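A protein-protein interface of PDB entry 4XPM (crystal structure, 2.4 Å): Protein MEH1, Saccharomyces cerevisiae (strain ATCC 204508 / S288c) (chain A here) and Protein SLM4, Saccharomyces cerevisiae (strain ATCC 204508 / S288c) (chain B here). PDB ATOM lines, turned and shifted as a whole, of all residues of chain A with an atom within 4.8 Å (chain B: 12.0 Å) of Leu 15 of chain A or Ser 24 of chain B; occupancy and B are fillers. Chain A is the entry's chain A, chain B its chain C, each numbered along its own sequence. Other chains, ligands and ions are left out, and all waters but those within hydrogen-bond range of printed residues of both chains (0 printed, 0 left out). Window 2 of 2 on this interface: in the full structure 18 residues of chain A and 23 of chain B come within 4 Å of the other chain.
Of the 11 printed residues of chain A, 4 touch a printed residue of chain B.
Among the printed residues, no Asp or Glu carboxylate lies within 4 Å of a Lys or Arg side-chain nitrogen of the other chain.
No residue of chain B comes within 4 Å of Leu 12 of chain A.
No residue of chain B comes within 4 Å of Lys 14 of chain A.
Leu 15 of chain A touches just these residues of chain B: Ser 24 and Val 25.
No residue of chain B comes within 4 Å of His 16 of chain A.
Ile 19 of chain A touches just one residue of chain B: Val 25.
Of the printed residues of chain B, Glu 22 of chain A touches Asp 21, Leu 22, His 23 and Ser 24.
Of the printed residues of chain A, Asp 21 of chain B touches Glu 22.
Of the printed residues of chain A, Leu 22 of chain B touches Glu 22 (3.3 Å).
Of the printed residues of chain A, His 23 of chain B touches Glu 22 (2.9 Å).
Ser 24 of chain B touches just these residues of chain A: Leu 15 (3.8 Å), Asn 18 (3.1 Å) and Glu 22 (2.5 Å).
Of the printed residues of chain A, Val 25 of chain B touches Leu 15 and Ile 19.
Phe 27 of chain B touches none of the printed residues of chain A.
The nearest residue of chain A that does not touch Ser 24 of chain B is Ile 19 of chain A (4.2 Å).
The nearest printed residue of chain A that does not touch Val 25 of chain B is Glu 22 of chain A (4.6 Å).
The side-chain carboxylate (OE1) of Glu 22 of chain A is in hydrogen-bond range of the side-chain hydroxyl (OG) of Ser 24 of chain B, 2.5 Å away.
The side-chain carboxylate (OE2) of Glu 22 of chain A lies within hydrogen-bond range of the backbone NH (N) of His 23 of chain B, at 2.9 Å.
O of Lys 14 of chain A lies close to ND2 of Asn 18 of chain A (3.5 Å).
The backbone NH (N) of Leu 22 of chain B sits at hydrogen-bond distance from the backbone carbonyl oxygen (O) of Phe 27 of chain B, 2.7 Å away.
Leu 15 of chain A touches Ser 24 of chain B.
Val 25 of chain B touches Leu 15 of chain A (CG1 to CD1, 3.9 Å).
Asn 18 of chain A touches Ser 24 of chain B (CB to OG, 3.1 Å).
Val 25 of chain B touches Ile 19 of chain A (CG1 to CD1, 3.9 Å).
Glu 22 of chain A touches Asp 21 of chain B (OE2 to O, 3.8 Å).
Glu 22 of chain A touches Leu 22 of chain B (OE2 to CA, 3.3 Å).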
ATOM      1  N   ILE A   7     -13.043 -10.013  23.393  1.00  0.00           N
ATOM      2  CA  ILE A   7     -13.423  -9.109  22.318  1.00  0.00           C
ATOM      3  C   ILE A   7     -14.925  -8.879  22.423  1.00  0.00           C
ATOM      4  O   ILE A   7     -15.702  -9.828  22.411  1.00  0.00           O
ATOM      5  CB  ILE A   7     -13.013  -9.644  20.912  1.00  0.00           C
ATOM      6  CG1 ILE A   7     -13.467  -8.673  19.817  1.00  0.00           C
ATOM      7  CG2 ILE A   7     -13.556 -11.059  20.665  1.00  0.00           C
ATOM      8  CD1 ILE A   7     -13.071  -9.094  18.415  1.00  0.00           C
ATOM      9  N   GLN A  11     -16.745  -4.416  19.234  1.00  0.00           N
ATOM     10  CA  GLN A  11     -15.427  -4.569  18.593  1.00  0.00           C
ATOM     11  C   GLN A  11     -15.458  -5.570  17.442  1.00  0.00           C
ATOM     12  O   GLN A  11     -14.862  -5.348  16.389  1.00  0.00           O
ATOM     13  CB  GLN A  11     -14.375  -5.033  19.605  1.00  0.00           C
ATOM     14  CG  GLN A  11     -13.777  -3.936  20.453  1.00  0.00           C
ATOM     15  CD  GLN A  11     -13.248  -4.468  21.777  1.00  0.00           C
ATOM     16  OE1 GLN A  11     -13.814  -5.400  22.350  1.00  0.00           O
ATOM     17  NE2 GLN A  11     -12.166  -3.877  22.267  1.00  0.00           N
ATOM     18  N   LEU A  12     -16.141  -6.684  17.673  1.00  0.00           N
ATOM     19  CA  LEU A  12     -16.200  -7.772  16.719  1.00  0.00           C
ATOM     20  C   LEU A  12     -16.926  -7.332  15.444  1.00  0.00           C
ATOM     21  O   LEU A  12     -16.435  -7.545  14.332  1.00  0.00           O
ATOM     22  CB  LEU A  12     -16.893  -8.971  17.365  1.00  0.00           C
ATOM     23  CG  LEU A  12     -17.195 -10.137  16.435  1.00  0.00           C
ATOM     24  CD1 LEU A  12     -15.916 -10.591  15.740  1.00  0.00           C
ATOM     25  CD2 LEU A  12     -17.864 -11.284  17.198  1.00  0.00           C
ATOM     26  N   LYS A  13     -18.088  -6.715  15.632  1.00  0.00           N
ATOM     27  CA  LYS A  13     -18.868  -6.113  14.559  1.00  0.00           C
ATOM     28  C   LYS A  13     -18.026  -5.077  13.800  1.00  0.00           C
ATOM     29  O   LYS A  13     -17.956  -5.078  12.560  1.00  0.00           O
ATOM     30  CB  LYS A  13     -20.095  -5.447  15.183  1.00  0.00           C
ATOM     31  CG  LYS A  13     -21.157  -4.961  14.218  1.00  0.00           C
ATOM     32  CD  LYS A  13     -22.450  -4.692  14.992  1.00  0.00           C
ATOM     33  CE  LYS A  13     -23.473  -3.947  14.154  1.00  0.00           C
ATOM     34  NZ  LYS A  13     -23.008  -2.574  13.800  1.00  0.00           N
ATOM     35  N   LYS A  14     -17.362  -4.212  14.558  1.00  0.00           N
ATOM     36  CA  LYS A  14     -16.520  -3.174  13.969  1.00  0.00           C
ATOM     37  C   LYS A  14     -15.373  -3.756  13.141  1.00  0.00           C
ATOM     38  O   LYS A  14     -15.052  -3.253  12.055  1.00  0.00           O
ATOM     39  CB  LYS A  14     -16.007  -2.217  15.057  1.00  0.00           C
ATOM     40  CG  LYS A  14     -15.092  -1.086  14.565  1.00  0.00           C
ATOM     41  CD  LYS A  14     -15.736  -0.235  13.466  1.00  0.00           C
ATOM     42  CE  LYS A  14     -14.882   1.013  13.192  1.00  0.00           C
ATOM     43  NZ  LYS A  14     -15.401   1.865  12.086  1.00  0.00           N
ATOM     44  N   LEU A  15     -14.766  -4.822  13.640  1.00  0.00           N
ATOM     45  CA  LEU A  15     -13.715  -5.487  12.894  1.00  0.00           C
ATOM     46  C   LEU A  15     -14.276  -6.136  11.615  1.00  0.00           C
ATOM     47  O   LEU A  15     -13.607  -6.196  10.587  1.00  0.00           O
ATOM     48  CB  LEU A  15     -13.021  -6.518  13.777  1.00  0.00           C
ATOM     49  CG  LEU A  15     -11.990  -7.405  13.084  1.00  0.00           C
ATOM     50  CD1 LEU A  15     -10.840  -6.581  12.527  1.00  0.00           C
ATOM     51  CD2 LEU A  15     -11.492  -8.454  14.058  1.00  0.00           C
ATOM     52  N   HIS A  16     -15.512  -6.614  11.680  1.00  0.00           N
ATOM     53  CA  HIS A  16     -16.153  -7.171  10.498  1.00  0.00           C
ATOM     54  C   HIS A  16     -16.335  -6.067   9.464  1.00  0.00           C
ATOM     55  O   HIS A  16     -15.996  -6.236   8.291  1.00  0.00           O
ATOM     56  CB  HIS A  16     -17.493  -7.790  10.887  1.00  0.00           C
ATOM     57  CG  HIS A  16     -18.276  -8.351   9.741  1.00  0.00           C
ATOM     58  ND1 HIS A  16     -19.035  -7.562   8.905  1.00  0.00           N
ATOM     59  CD2 HIS A  16     -18.464  -9.632   9.327  1.00  0.00           C
ATOM     60  CE1 HIS A  16     -19.646  -8.331   8.017  1.00  0.00           C
ATOM     61  NE2 HIS A  16     -19.316  -9.590   8.251  1.00  0.00           N
ATOM     62  N   SER A  17     -16.841  -4.919   9.899  1.00  0.00           N
ATOM     63  CA  SER A  17     -17.057  -3.807   8.968  1.00  0.00           C
ATOM     64  C   SER A  17     -15.745  -3.311   8.341  1.00  0.00           C
ATOM     65  O   SER A  17     -15.720  -2.960   7.158  1.00  0.00           O
ATOM     66  CB  SER A  17     -17.846  -2.661   9.628  1.00  0.00           C
ATOM     67  OG  SER A  17     -17.068  -1.487   9.757  1.00  0.00           O
ATOM     68  N   ASN A  18     -14.664  -3.292   9.128  1.00  0.00           N
ATOM     69  CA  ASN A  18     -13.347  -2.864   8.631  1.00  0.00           C
ATOM     70  C   ASN A  18     -12.806  -3.788   7.542  1.00  0.00           C
ATOM     71  O   ASN A  18     -12.380  -3.324   6.481  1.00  0.00           O
ATOM     72  CB  ASN A  18     -12.333  -2.703   9.779  1.00  0.00           C
ATOM     73  CG  ASN A  18     -12.665  -1.526  10.677  1.00  0.00           C
ATOM     74  OD1 ASN A  18     -13.479  -0.662  10.315  1.00  0.00           O
ATOM     75  ND2 ASN A  18     -12.049  -1.481  11.855  1.00  0.00           N
ATOM     76  N   ILE A  19     -12.832  -5.091   7.796  1.00  0.00           N
ATOM     77  CA  ILE A  19     -12.415  -6.059   6.788  1.00  0.00           C
ATOM     78  C   ILE A  19     -13.226  -5.873   5.487  1.00  0.00           C
ATOM     79  O   ILE A  19     -12.650  -5.805   4.397  1.00  0.00           O
ATOM     80  CB  ILE A  19     -12.538  -7.504   7.334  1.00  0.00           C
ATOM     81  CG1 ILE A  19     -11.659  -7.674   8.582  1.00  0.00           C
ATOM     82  CG2 ILE A  19     -12.152  -8.539   6.275  1.00  0.00           C
ATOM     83  CD1 ILE A  19     -11.815  -9.037   9.250  1.00  0.00           C
ATOM     84  N   GLU A  22     -12.369  -2.531   3.672  1.00  0.00           N
ATOM     85  CA  GLU A  22     -11.053  -2.573   3.043  1.00  0.00           C
ATOM     86  C   GLU A  22     -11.113  -3.390   1.765  1.00  0.00           C
ATOM     87  O   GLU A  22     -10.576  -2.983   0.744  1.00  0.00           O
ATOM     88  CB  GLU A  22      -9.995  -3.182   3.968  1.00  0.00           C
ATOM     89  CG  GLU A  22      -9.515  -2.290   5.102  1.00  0.00           C
ATOM     90  CD  GLU A  22      -8.164  -2.743   5.676  1.00  0.00           C
ATOM     91  OE1 GLU A  22      -8.160  -3.347   6.768  1.00  0.00           O
ATOM     92  OE2 GLU A  22      -7.107  -2.496   5.039  1.00  0.00           O
ATOM     93  N   TYR B  20      -4.669  -7.767  -2.553  1.00  0.00           N
ATOM     94  CA  TYR B  20      -5.326  -7.138  -1.417  1.00  0.00           C
ATOM     95  C   TYR B  20      -4.293  -6.969  -0.308  1.00  0.00           C
ATOM     96  O   TYR B  20      -3.392  -7.803  -0.156  1.00  0.00           O
ATOM     97  CB  TYR B  20      -6.476  -8.005  -0.908  1.00  0.00           C
ATOM     98  CG  TYR B  20      -7.673  -8.021  -1.816  1.00  0.00           C
ATOM     99  CD1 TYR B  20      -8.630  -7.024  -1.741  1.00  0.00           C
ATOM    100  CD2 TYR B  20      -7.845  -9.030  -2.742  1.00  0.00           C
ATOM    101  CE1 TYR B  20      -9.724  -7.033  -2.560  1.00  0.00           C
ATOM    102  CE2 TYR B  20      -8.931  -9.049  -3.565  1.00  0.00           C
ATOM    103  CZ  TYR B  20      -9.873  -8.049  -3.472  1.00  0.00           C
ATOM    104  OH  TYR B  20     -10.974  -8.076  -4.297  1.00  0.00           O
ATOM    105  N   ASP B  21      -4.410  -5.897   0.466  1.00  0.00           N
ATOM    106  CA  ASP B  21      -3.472  -5.663   1.562  1.00  0.00           C
ATOM    107  C   ASP B  21      -4.220  -5.004   2.689  1.00  0.00           C
ATOM    108  O   ASP B  21      -4.429  -3.793   2.677  1.00  0.00           O
ATOM    109  CB  ASP B  21      -2.330  -4.759   1.121  1.00  0.00           C
ATOM    110  CG  ASP B  21      -1.157  -4.786   2.083  1.00  0.00           C
ATOM    111  OD1 ASP B  21      -1.335  -5.179   3.256  1.00  0.00           O
ATOM    112  OD2 ASP B  21      -0.046  -4.408   1.657  1.00  0.00           O
ATOM    113  N   LEU B  22      -4.616  -5.811   3.662  1.00  0.00           N
ATOM    114  CA  LEU B  22      -5.485  -5.353   4.733  1.00  0.00           C
ATOM    115  C   LEU B  22      -4.645  -4.902   5.917  1.00  0.00           C
ATOM    116  O   LEU B  22      -3.532  -5.388   6.126  1.00  0.00           O
ATOM    117  CB  LEU B  22      -6.448  -6.471   5.137  1.00  0.00           C
ATOM    118  CG  LEU B  22      -7.745  -6.626   4.324  1.00  0.00           C
ATOM    119  CD1 LEU B  22      -7.560  -6.402   2.841  1.00  0.00           C
ATOM    120  CD2 LEU B  22      -8.374  -7.991   4.557  1.00  0.00           C
ATOM    121  N   HIS B  23      -5.150  -3.941   6.675  1.00  0.00           N
ATOM    122  CA  HIS B  23      -4.459  -3.554   7.891  1.00  0.00           C
ATOM    123  C   HIS B  23      -5.323  -3.824   9.113  1.00  0.00           C
ATOM    124  O   HIS B  23      -4.805  -3.929  10.223  1.00  0.00           O
ATOM    125  CB  HIS B  23      -3.978  -2.096   7.840  1.00  0.00           C
ATOM    126  CG  HIS B  23      -5.080  -1.096   7.679  1.00  0.00           C
ATOM    127  ND1 HIS B  23      -5.364  -0.489   6.474  1.00  0.00           N
ATOM    128  CD2 HIS B  23      -5.970  -0.598   8.572  1.00  0.00           C
ATOM    129  CE1 HIS B  23      -6.379   0.340   6.630  1.00  0.00           C
ATOM    130  NE2 HIS B  23      -6.767   0.292   7.893  1.00  0.00           N
ATOM    131  N   SER B  24      -6.633  -3.950   8.910  1.00  0.00           N
ATOM    132  CA  SER B  24      -7.547  -4.276  10.015  1.00  0.00           C
ATOM    133  C   SER B  24      -7.169  -5.609  10.641  1.00  0.00           C
ATOM    134  O   SER B  24      -7.184  -5.762  11.843  1.00  0.00           O
ATOM    135  CB  SER B  24      -8.993  -4.322   9.536  1.00  0.00           C
ATOM    136  OG  SER B  24      -9.356  -3.092   8.941  1.00  0.00           O
ATOM    137  N   VAL B  25      -6.837  -6.572   9.801  1.00  0.00           N
ATOM    138  CA  VAL B  25      -6.205  -7.793  10.251  1.00  0.00           C
ATOM    139  C   VAL B  25      -4.906  -7.859   9.470  1.00  0.00           C
ATOM    140  O   VAL B  25      -4.737  -7.159   8.460  1.00  0.00           O
ATOM    141  CB  VAL B  25      -7.099  -9.049   9.982  1.00  0.00           C
ATOM    142  CG1 VAL B  25      -8.304  -9.040  10.883  1.00  0.00           C
ATOM    143  CG2 VAL B  25      -7.550  -9.105   8.544  1.00  0.00           C
ATOM    144  N   ASP B  26      -3.970  -8.676   9.919  1.00  0.00           N
ATOM    145  CA  ASP B  26      -2.678  -8.711   9.241  1.00  0.00           C
ATOM    146  C   ASP B  26      -2.733  -9.646   8.038  1.00  0.00           C
ATOM    147  O   ASP B  26      -2.207 -10.759   8.080  1.00  0.00           O
ATOM    148  CB  ASP B  26      -1.569  -9.124  10.208  1.00  0.00           C
ATOM    149  CG  ASP B  26      -0.191  -8.750   9.702  1.00  0.00           C
ATOM    150  OD1 ASP B  26      -0.098  -8.157   8.604  1.00  0.00           O
ATOM    151  OD2 ASP B  26       0.799  -9.037  10.410  1.00  0.00           O
ATOM    152  N   PHE B  27      -3.373  -9.199   6.964  1.00  0.00           N
ATOM    153  CA  PHE B  27      -3.607 -10.094   5.839  1.00  0.00           C
ATOM    154  C   PHE B  27      -3.313  -9.448   4.499  1.00  0.00           C
ATOM    155  O   PHE B  27      -3.676  -8.304   4.245  1.00  0.00           O
ATOM    156  CB  PHE B  27      -5.044 -10.632   5.854  1.00  0.00           C
ATOM    157  CG  PHE B  27      -5.385 -11.499   4.665  1.00  0.00           C
ATOM    158  CD1 PHE B  27      -5.109 -12.861   4.684  1.00  0.00           C
ATOM    159  CD2 PHE B  27      -5.986 -10.954   3.533  1.00  0.00           C
ATOM    160  CE1 PHE B  27      -5.430 -13.661   3.598  1.00  0.00           C
ATOM    161  CE2 PHE B  27      -6.314 -11.744   2.448  1.00  0.00           C
ATOM    162  CZ  PHE B  27      -6.039 -13.102   2.476  1.00  0.00           C
ATOM    163  N   LYS B  28      -2.688 -10.219   3.629  1.00  0.00           N
ATOM    164  CA  LYS B  28      -2.243  -9.714   2.344  1.00  0.00           C
ATOM    165  C   LYS B  28      -2.159 -10.885   1.381  1.00  0.00           C
ATOM    166  O   LYS B  28      -1.692 -11.963   1.751  1.00  0.00           O
ATOM    167  CB  LYS B  28      -0.876  -9.065   2.513  1.00  0.00           C
ATOM    168  CG  LYS B  28      -0.106  -8.843   1.235  1.00  0.00           C
ATOM    169  CD  LYS B  28       1.356  -8.520   1.535  1.00  0.00           C
ATOM    170  CE  LYS B  28       1.991  -9.595   2.427  1.00  0.00           C
ATOM    171  NZ  LYS B  28       1.899 -10.971   1.840  1.00  0.00           N
ATOM    172  N   THR B  29      -2.631 -10.688   0.156  1.00  0.00           N
ATOM    173  CA  THR B  29      -2.475 -11.712  -0.871  1.00  0.00           C
ATOM    174  C   THR B  29      -1.287 -11.356  -1.721  1.00  0.00           C
ATOM    175  O   THR B  29      -0.792 -10.229  -1.668  1.00  0.00           O
ATOM    176  CB  THR B  29      -3.698 -11.807  -1.796  1.00  0.00           C
ATOM    177  OG1 THR B  29      -3.758 -10.651  -2.650  1.00  0.00           O
ATOM    178  CG2 THR B  29      -4.979 -11.920  -0.974  1.00  0.00           C
